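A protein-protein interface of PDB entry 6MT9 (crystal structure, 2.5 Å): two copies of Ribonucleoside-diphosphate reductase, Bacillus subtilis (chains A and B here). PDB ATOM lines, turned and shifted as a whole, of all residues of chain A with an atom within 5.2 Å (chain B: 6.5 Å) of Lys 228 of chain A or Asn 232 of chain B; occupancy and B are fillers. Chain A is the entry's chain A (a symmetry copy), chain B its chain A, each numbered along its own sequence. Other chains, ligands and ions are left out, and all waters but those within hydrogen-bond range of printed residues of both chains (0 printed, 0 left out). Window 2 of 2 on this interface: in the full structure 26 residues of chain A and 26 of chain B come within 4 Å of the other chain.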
ATOM      1  N   VAL A 223       4.793  13.515  35.346  1.00  0.00           N
ATOM      2  CA  VAL A 223       6.063  13.104  35.933  1.00  0.00           C
ATOM      3  C   VAL A 223       7.017  12.574  34.862  1.00  0.00           C
ATOM      4  O   VAL A 223       8.224  12.842  34.899  1.00  0.00           O
ATOM      5  CB  VAL A 223       5.795  12.074  37.044  1.00  0.00           C
ATOM      6  CG1 VAL A 223       7.053  11.359  37.425  1.00  0.00           C
ATOM      7  CG2 VAL A 223       5.190  12.773  38.254  1.00  0.00           C
ATOM      8  N   VAL A 224       6.496  11.828  33.882  1.00  0.00           N
ATOM      9  CA  VAL A 224       7.381  11.235  32.880  1.00  0.00           C
ATOM     10  C   VAL A 224       8.105  12.309  32.077  1.00  0.00           C
ATOM     11  O   VAL A 224       9.251  12.110  31.654  1.00  0.00           O
ATOM     12  CB  VAL A 224       6.591  10.282  31.964  1.00  0.00           C
ATOM     13  CG1 VAL A 224       7.523   9.659  30.932  1.00  0.00           C
ATOM     14  CG2 VAL A 224       5.929   9.201  32.796  1.00  0.00           C
ATOM     15  N   GLY A 225       7.465  13.462  31.862  1.00  0.00           N
ATOM     16  CA  GLY A 225       8.135  14.543  31.158  1.00  0.00           C
ATOM     17  C   GLY A 225       9.354  15.052  31.903  1.00  0.00           C
ATOM     18  O   GLY A 225      10.403  15.301  31.302  1.00  0.00           O
ATOM     19  N   VAL A 226       9.240  15.199  33.226  1.00  0.00           N
ATOM     20  CA  VAL A 226      10.380  15.672  34.001  1.00  0.00           C
ATOM     21  C   VAL A 226      11.441  14.584  34.119  1.00  0.00           C
ATOM     22  O   VAL A 226      12.642  14.883  34.167  1.00  0.00           O
ATOM     23  CB  VAL A 226       9.911  16.178  35.376  1.00  0.00           C
ATOM     24  CG1 VAL A 226      11.087  16.686  36.187  1.00  0.00           C
ATOM     25  CG2 VAL A 226       8.888  17.284  35.191  1.00  0.00           C
ATOM     26  N   MET A 227      11.032  13.311  34.140  1.00  0.00           N
ATOM     27  CA  MET A 227      12.008  12.223  34.149  1.00  0.00           C
ATOM     28  C   MET A 227      12.870  12.246  32.895  1.00  0.00           C
ATOM     29  O   MET A 227      14.077  11.970  32.951  1.00  0.00           O
ATOM     30  CB  MET A 227      11.303  10.875  34.274  1.00  0.00           C
ATOM     31  CG  MET A 227      10.493  10.707  35.536  1.00  0.00           C
ATOM     32  SD  MET A 227       9.605   9.141  35.542  1.00  0.00           S
ATOM     33  CE  MET A 227      10.948   7.976  35.811  1.00  0.00           C
ATOM     34  N   LYS A 228      12.264  12.579  31.751  1.00  0.00           N
ATOM     35  CA  LYS A 228      13.013  12.640  30.502  1.00  0.00           C
ATOM     36  C   LYS A 228      14.053  13.750  30.545  1.00  0.00           C
ATOM     37  O   LYS A 228      15.204  13.548  30.140  1.00  0.00           O
ATOM     38  CB  LYS A 228      12.051  12.825  29.326  1.00  0.00           C
ATOM     39  CG  LYS A 228      12.615  12.384  27.991  1.00  0.00           C
ATOM     40  CD  LYS A 228      12.857  10.871  27.972  1.00  0.00           C
ATOM     41  CE  LYS A 228      14.079  10.497  27.125  1.00  0.00           C
ATOM     42  NZ  LYS A 228      15.355  11.030  27.714  1.00  0.00           N
ATOM     43  N   LEU A 229      13.679  14.923  31.060  1.00  0.00           N
ATOM     44  CA  LEU A 229      14.652  15.999  31.240  1.00  0.00           C
ATOM     45  C   LEU A 229      15.771  15.572  32.184  1.00  0.00           C
ATOM     46  O   LEU A 229      16.954  15.784  31.897  1.00  0.00           O
ATOM     47  CB  LEU A 229      13.951  17.261  31.760  1.00  0.00           C
ATOM     48  CG  LEU A 229      12.987  17.982  30.810  1.00  0.00           C
ATOM     49  CD1 LEU A 229      12.183  19.056  31.537  1.00  0.00           C
ATOM     50  CD2 LEU A 229      13.747  18.594  29.656  1.00  0.00           C
ATOM     51  N   LEU A 230      15.416  14.968  33.323  1.00  0.00           N
ATOM     52  CA  LEU A 230      16.433  14.539  34.280  1.00  0.00           C
ATOM     53  C   LEU A 230      17.329  13.462  33.688  1.00  0.00           C
ATOM     54  O   LEU A 230      18.552  13.493  33.861  1.00  0.00           O
ATOM     55  CB  LEU A 230      15.768  14.029  35.556  1.00  0.00           C
ATOM     56  CG  LEU A 230      15.061  15.071  36.408  1.00  0.00           C
ATOM     57  CD1 LEU A 230      14.123  14.369  37.369  1.00  0.00           C
ATOM     58  CD2 LEU A 230      16.085  15.922  37.154  1.00  0.00           C
ATOM     59  N   ASP A 231      16.731  12.489  32.997  1.00  0.00           N
ATOM     60  CA  ASP A 231      17.517  11.447  32.355  1.00  0.00           C
ATOM     61  C   ASP A 231      18.612  12.056  31.503  1.00  0.00           C
ATOM     62  O   ASP A 231      19.774  11.642  31.575  1.00  0.00           O
ATOM     63  CB  ASP A 231      16.598  10.559  31.516  1.00  0.00           C
ATOM     64  CG  ASP A 231      17.345   9.472  30.781  1.00  0.00           C
ATOM     65  OD1 ASP A 231      18.080   8.701  31.437  1.00  0.00           O
ATOM     66  OD2 ASP A 231      17.188   9.383  29.545  1.00  0.00           O
ATOM     67  N   ASN A 232      18.264  13.087  30.734  1.00  0.00           N
ATOM     68  CA  ASN A 232      19.234  13.757  29.880  1.00  0.00           C
ATOM     69  C   ASN A 232      20.258  14.541  30.681  1.00  0.00           C
ATOM     70  O   ASN A 232      21.437  14.587  30.304  1.00  0.00           O
ATOM     71  CB  ASN A 232      18.515  14.681  28.919  1.00  0.00           C
ATOM     72  CG  ASN A 232      18.551  14.163  27.538  1.00  0.00           C
ATOM     73  OD1 ASN A 232      17.518  13.789  26.979  1.00  0.00           O
ATOM     74  ND2 ASN A 232      19.758  14.080  26.976  1.00  0.00           N
ATOM     75  N   ALA A 233      19.824  15.198  31.758  1.00  0.00           N
ATOM     76  CA  ALA A 233      20.758  15.931  32.604  1.00  0.00           C
ATOM     77  C   ALA A 233      21.846  15.007  33.143  1.00  0.00           C
ATOM     78  O   ALA A 233      23.036  15.333  33.091  1.00  0.00           O
ATOM     79  CB  ALA A 233      20.002  16.613  33.744  1.00  0.00           C
ATOM     80  N   GLU A 271      10.972   3.905  22.956  1.00  0.00           N
ATOM     81  CA  GLU A 271      11.979   4.935  23.194  1.00  0.00           C
ATOM     82  C   GLU A 271      11.375   6.321  23.390  1.00  0.00           C
ATOM     83  O   GLU A 271      12.052   7.201  23.933  1.00  0.00           O
ATOM     84  CB  GLU A 271      12.986   4.968  22.042  1.00  0.00           C
ATOM     85  CG  GLU A 271      13.620   3.621  21.714  1.00  0.00           C
ATOM     86  CD  GLU A 271      14.303   2.973  22.909  1.00  0.00           C
ATOM     87  OE1 GLU A 271      13.797   1.939  23.402  1.00  0.00           O
ATOM     88  OE2 GLU A 271      15.348   3.494  23.358  1.00  0.00           O
ATOM     89  N   ASP A 272      10.129   6.539  22.957  1.00  0.00           N
ATOM     90  CA  ASP A 272       9.474   7.821  23.213  1.00  0.00           C
ATOM     91  C   ASP A 272       9.336   8.091  24.707  1.00  0.00           C
ATOM     92  O   ASP A 272       9.403   9.248  25.141  1.00  0.00           O
ATOM     93  CB  ASP A 272       8.102   7.856  22.537  1.00  0.00           C
ATOM     94  N   VAL A 273       9.160   7.037  25.505  1.00  0.00           N
ATOM     95  CA  VAL A 273       8.989   7.129  26.951  1.00  0.00           C
ATOM     96  C   VAL A 273      10.168   6.531  27.711  1.00  0.00           C
ATOM     97  O   VAL A 273      10.201   6.601  28.949  1.00  0.00           O
ATOM     98  CB  VAL A 273       7.659   6.468  27.381  1.00  0.00           C
ATOM     99  CG1 VAL A 273       7.265   6.845  28.798  1.00  0.00           C
ATOM    100  CG2 VAL A 273       6.539   6.860  26.420  1.00  0.00           C
ATOM    101  N   ARG A 274      11.155   5.975  27.012  1.00  0.00           N
ATOM    102  CA  ARG A 274      12.227   5.251  27.681  1.00  0.00           C
ATOM    103  C   ARG A 274      13.131   6.197  28.458  1.00  0.00           C
ATOM    104  O   ARG A 274      13.487   7.282  27.988  1.00  0.00           O
ATOM    105  CB  ARG A 274      13.057   4.461  26.668  1.00  0.00           C
ATOM    106  N   VAL A 275      13.493   5.772  29.664  1.00  0.00           N
ATOM    107  CA  VAL A 275      14.456   6.458  30.515  1.00  0.00           C
ATOM    108  C   VAL A 275      15.517   5.436  30.880  1.00  0.00           C
ATOM    109  O   VAL A 275      15.183   4.363  31.395  1.00  0.00           O
ATOM    110  CB  VAL A 275      13.794   7.030  31.784  1.00  0.00           C
ATOM    111  CG1 VAL A 275      14.845   7.508  32.733  1.00  0.00           C
ATOM    112  CG2 VAL A 275      12.845   8.164  31.432  1.00  0.00           C
ATOM    113  N   MET B 190      13.025  27.542  27.989  1.00  0.00           N
ATOM    114  CA  MET B 190      11.714  27.041  28.374  1.00  0.00           C
ATOM    115  C   MET B 190      10.806  28.170  28.834  1.00  0.00           C
ATOM    116  O   MET B 190       9.593  28.127  28.598  1.00  0.00           O
ATOM    117  CB  MET B 190      11.844  25.976  29.464  1.00  0.00           C
ATOM    118  CG  MET B 190      12.509  24.699  28.988  1.00  0.00           C
ATOM    119  SD  MET B 190      12.228  23.273  30.055  1.00  0.00           S
ATOM    120  CE  MET B 190      12.921  23.836  31.608  1.00  0.00           C
ATOM    121  N   MET B 227      22.964  20.752  22.521  1.00  0.00           N
ATOM    122  CA  MET B 227      21.819  20.708  21.613  1.00  0.00           C
ATOM    123  C   MET B 227      20.805  19.663  22.057  1.00  0.00           C
ATOM    124  O   MET B 227      19.589  19.877  21.951  1.00  0.00           O
ATOM    125  CB  MET B 227      22.280  20.416  20.188  1.00  0.00           C
ATOM    126  CG  MET B 227      23.218  21.447  19.610  1.00  0.00           C
ATOM    127  SD  MET B 227      23.801  20.962  17.977  1.00  0.00           S
ATOM    128  CE  MET B 227      22.322  21.218  16.986  1.00  0.00           C
ATOM    129  N   LYS B 228      21.290  18.525  22.562  1.00  0.00           N
ATOM    130  CA  LYS B 228      20.393  17.473  23.024  1.00  0.00           C
ATOM    131  C   LYS B 228      19.589  17.936  24.230  1.00  0.00           C
ATOM    132  O   LYS B 228      18.374  17.712  24.297  1.00  0.00           O
ATOM    133  CB  LYS B 228      21.195  16.208  23.344  1.00  0.00           C
ATOM    134  CG  LYS B 228      20.375  14.934  23.318  1.00  0.00           C
ATOM    135  CD  LYS B 228      19.863  14.641  21.904  1.00  0.00           C
ATOM    136  CE  LYS B 228      18.486  13.970  21.921  1.00  0.00           C
ATOM    137  NZ  LYS B 228      17.425  14.878  22.475  1.00  0.00           N
ATOM    138  N   LEU B 229      20.238  18.610  25.180  1.00  0.00           N
ATOM    139  CA  LEU B 229      19.511  19.185  26.311  1.00  0.00           C
ATOM    140  C   LEU B 229      18.480  20.204  25.837  1.00  0.00           C
ATOM    141  O   LEU B 229      17.326  20.187  26.278  1.00  0.00           O
ATOM    142  CB  LEU B 229      20.495  19.825  27.300  1.00  0.00           C
ATOM    143  CG  LEU B 229      21.428  18.890  28.080  1.00  0.00           C
ATOM    144  CD1 LEU B 229      22.508  19.669  28.824  1.00  0.00           C
ATOM    145  CD2 LEU B 229      20.634  18.047  29.051  1.00  0.00           C
ATOM    146  N   LEU B 230      18.880  21.107  24.935  1.00  0.00           N
ATOM    147  CA  LEU B 230      17.951  22.120  24.441  1.00  0.00           C
ATOM    148  C   LEU B 230      16.799  21.486  23.676  1.00  0.00           C
ATOM    149  O   LEU B 230      15.639  21.880  23.840  1.00  0.00           O
ATOM    150  CB  LEU B 230      18.688  23.118  23.553  1.00  0.00           C
ATOM    151  CG  LEU B 230      19.687  24.029  24.250  1.00  0.00           C
ATOM    152  CD1 LEU B 230      20.610  24.636  23.213  1.00  0.00           C
ATOM    153  CD2 LEU B 230      18.950  25.110  25.037  1.00  0.00           C
ATOM    154  N   ASP B 231      17.106  20.509  22.819  1.00  0.00           N
ATOM    155  CA  ASP B 231      16.062  19.815  22.083  1.00  0.00           C
ATOM    156  C   ASP B 231      14.984  19.323  23.027  1.00  0.00           C
ATOM    157  O   ASP B 231      13.789  19.514  22.780  1.00  0.00           O
ATOM    158  CB  ASP B 231      16.675  18.656  21.298  1.00  0.00           C
ATOM    159  CG  ASP B 231      15.646  17.856  20.535  1.00  0.00           C
ATOM    160  OD1 ASP B 231      14.887  18.456  19.744  1.00  0.00           O
ATOM    161  OD2 ASP B 231      15.606  16.621  20.721  1.00  0.00           O
ATOM    162  N   ASN B 232      15.399  18.738  24.152  1.00  0.00           N
ATOM    163  CA  ASN B 232      14.453  18.234  25.137  1.00  0.00           C
ATOM    164  C   ASN B 232      13.712  19.353  25.846  1.00  0.00           C
ATOM    165  O   ASN B 232      12.520  19.214  26.149  1.00  0.00           O
ATOM    166  CB  ASN B 232      15.181  17.375  26.150  1.00  0.00           C
ATOM    167  CG  ASN B 232      14.856  15.946  25.985  1.00  0.00           C
ATOM    168  OD1 ASN B 232      15.713  15.144  25.611  1.00  0.00           O
ATOM    169  ND2 ASN B 232      13.586  15.606  26.212  1.00  0.00           N
ATOM    170  N   ALA B 233      14.408  20.449  26.159  1.00  0.00           N
ATOM    171  CA  ALA B 233      13.753  21.585  26.797  1.00  0.00           C
ATOM    172  C   ALA B 233      12.605  22.104  25.936  1.00  0.00           C
ATOM    173  O   ALA B 233      11.498  22.338  26.433  1.00  0.00           O
ATOM    174  CB  ALA B 233      14.775  22.686  27.073  1.00  0.00           C
ATOM    175  N   PHE B 234      12.845  22.271  24.632  1.00  0.00           N
ATOM    176  CA  PHE B 234      11.780  22.731  23.744  1.00  0.00           C
ATOM    177  C   PHE B 234      10.661  21.701  23.613  1.00  0.00           C
ATOM    178  O   PHE B 234       9.497  22.080  23.448  1.00  0.00           O
ATOM    179  CB  PHE B 234      12.356  23.087  22.372  1.00  0.00           C
ATOM    180  CG  PHE B 234      13.195  24.330  22.382  1.00  0.00           C
ATOM    181  CD1 PHE B 234      12.629  25.557  22.667  1.00  0.00           C
ATOM    182  CD2 PHE B 234      14.547  24.273  22.110  1.00  0.00           C
ATOM    183  CE1 PHE B 234      13.398  26.710  22.688  1.00  0.00           C
ATOM    184  CE2 PHE B 234      15.319  25.420  22.124  1.00  0.00           C
ATOM    185  CZ  PHE B 234      14.744  26.641  22.414  1.00  0.00           C
ATOM    186  N   ARG B 235      10.982  20.405  23.685  1.00  0.00           N
ATOM    187  CA  ARG B 235       9.935  19.386  23.670  1.00  0.00           C
ATOM    188  C   ARG B 235       9.018  19.517  24.879  1.00  0.00           C
ATOM    189  O   ARG B 235       7.791  19.472  24.750  1.00  0.00           O
ATOM    190  CB  ARG B 235      10.545  17.989  23.659  1.00  0.00           C
ATOM    191  CG  ARG B 235      11.103  17.522  22.353  1.00  0.00           C
ATOM    192  CD  ARG B 235      11.389  16.041  22.474  1.00  0.00           C
ATOM    193  NE  ARG B 235      12.320  15.568  21.461  1.00  0.00           N
ATOM    194  CZ  ARG B 235      11.970  15.240  20.222  1.00  0.00           C
ATOM    195  NH1 ARG B 235      10.702  15.350  19.835  1.00  0.00           N
ATOM    196  NH2 ARG B 235      12.891  14.804  19.370  1.00  0.00           N
ATOM    197  N   TYR B 236       9.603  19.647  26.072  1.00  0.00           N
ATOM    198  CA  TYR B 236       8.811  19.676  27.296  1.00  0.00           C
ATOM    199  C   TYR B 236       7.892  20.898  27.342  1.00  0.00           C
ATOM    200  O   TYR B 236       6.685  20.772  27.578  1.00  0.00           O
ATOM    201  CB  TYR B 236       9.744  19.638  28.511  1.00  0.00           C
ATOM    202  CG  TYR B 236       9.009  19.722  29.821  1.00  0.00           C
ATOM    203  CD1 TYR B 236       8.436  18.594  30.381  1.00  0.00           C
ATOM    204  CD2 TYR B 236       8.880  20.930  30.495  1.00  0.00           C
ATOM    205  CE1 TYR B 236       7.748  18.658  31.564  1.00  0.00           C
ATOM    206  CE2 TYR B 236       8.194  21.004  31.688  1.00  0.00           C
ATOM    207  CZ  TYR B 236       7.628  19.863  32.216  1.00  0.00           C
ATOM    208  OH  TYR B 236       6.935  19.909  33.405  1.00  0.00           O
ATOM    209  N   ALA B 237       8.436  22.088  27.096  1.00  0.00           N
ATOM    210  CA  ALA B 237       7.708  23.336  27.326  1.00  0.00           C
ATOM    211  C   ALA B 237       6.962  23.758  26.063  1.00  0.00           C
ATOM    212  O   ALA B 237       7.570  24.269  25.118  1.00  0.00           O
ATOM    213  CB  ALA B 237       8.671  24.433  27.778  1.00  0.00           C
ATOM    214  N   THR B 277      13.654  18.967  17.124  1.00  0.00           N
ATOM    215  CA  THR B 277      12.877  20.199  17.182  1.00  0.00           C
ATOM    216  C   THR B 277      13.733  21.453  17.051  1.00  0.00           C
ATOM    217  O   THR B 277      13.209  22.563  17.219  1.00  0.00           O
ATOM    218  CB  THR B 277      12.062  20.271  18.480  1.00  0.00           C
ATOM    219  OG1 THR B 277      12.846  20.883  19.517  1.00  0.00           O
ATOM    220  CG2 THR B 277      11.631  18.882  18.916  1.00  0.00           C
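Lys 228 of chain A touches just one residue of chain B: Asn 232 (3.8 Å).
Asn 232 of chain B touches just these residues of chain A: Lys 228, Leu 229 and Asn 232.
Of the printed residues of chain A, Tyr 236 of chain B touches Gly 225 (3.9 Å), Val 226 (3.7 Å) and Leu 229 (3.7 Å).
Of the printed residues of chain A, Leu 229 of chain B touches Asn 232.
Of the printed residues of chain B, Gly 225 of chain A touches Tyr 236 (3.9 Å).
Of the printed residues of chain B, Asn 232 of chain A touches Lys 228 (3.8 Å), Leu 229 (3.8 Å) and Asn 232 (2.6 Å).
Of the printed residues of chain B, Val 226 of chain A touches Tyr 236.
Ala 233 of chain A touches none of the printed residues of chain B.
Val 223 of chain A touches none of the printed residues of chain B.
The nearest printed residue of chain B that does not touch Lys 228 of chain A is Arg 235 of chain B (6.7 Å).
The nearest printed residue of chain A that does not touch Asn 232 of chain B is Gly 225 of chain A (6.0 Å).
The nearest printed residue of chain B that does not touch Leu 229 of chain A is Ala 233 of chain B (4.01 Å).
NZ of Lys 228 of chain B is in salt-bridge range of OD2 of Asp 231 of chain B (3.1 Å).
OD2 of Asp 231 of chain A is in salt-bridge range of NZ of Lys 228 of chain A (3.1 Å).
Hydrophobic or aromatic side chains of chain B that line the printed part of chain A: Leu 229 and Tyr 236.
Along chain B the printed residues that touch a printed residue of chain A span positions 228 to 236.
Hydrophobic or aromatic side chains of chain A that line the printed part of chain B: Val 226 and Leu 229.
Among the printed residues, no Asp or Glu carboxylate lies within 4 Å of a Lys or Arg side-chain nitrogen of the other chain.
OD1 of Asn 232 of chain B lies close to OD1 of Asn 232 of chain A (2.6 Å).
Lys 228 of chain A touches Asn 232 of chain B, and with the chains exchanged Asn 232 of chain A touches Lys 228 of chain B.
Leu 229 of chain A touches Asn 232 of chain B, and with the chains exchanged Asn 232 of chain A touches Leu 229 of chain B.
Asn 232 of chain A touches its own counterpart, Asn 232 of chain B.
7 positions are printed for both chains.
Of the 8 pairs that touch across the chains among the printed residues, 5 have their exchanged pair printed and touching as well.
Among the printed residues, merely in contact across the chains: Gly 225 of chain A with Tyr 236 of chain B (3.9 Å), Val 226 of chain A with Tyr 236 of chain B (3.7 Å), Lys 228 of chain A with Asn 232 of chain B (3.8 Å), Leu 229 of chain A with Asn 232 of chain B (3.8 Å), Leu 229 of chain A with Tyr 236 of chain B (3.7 Å), Asn 232 of chain A with Lys 228 of chain B (3.8 Å) and Asn 232 of chain A with Leu 229 of chain B (3.8 Å).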
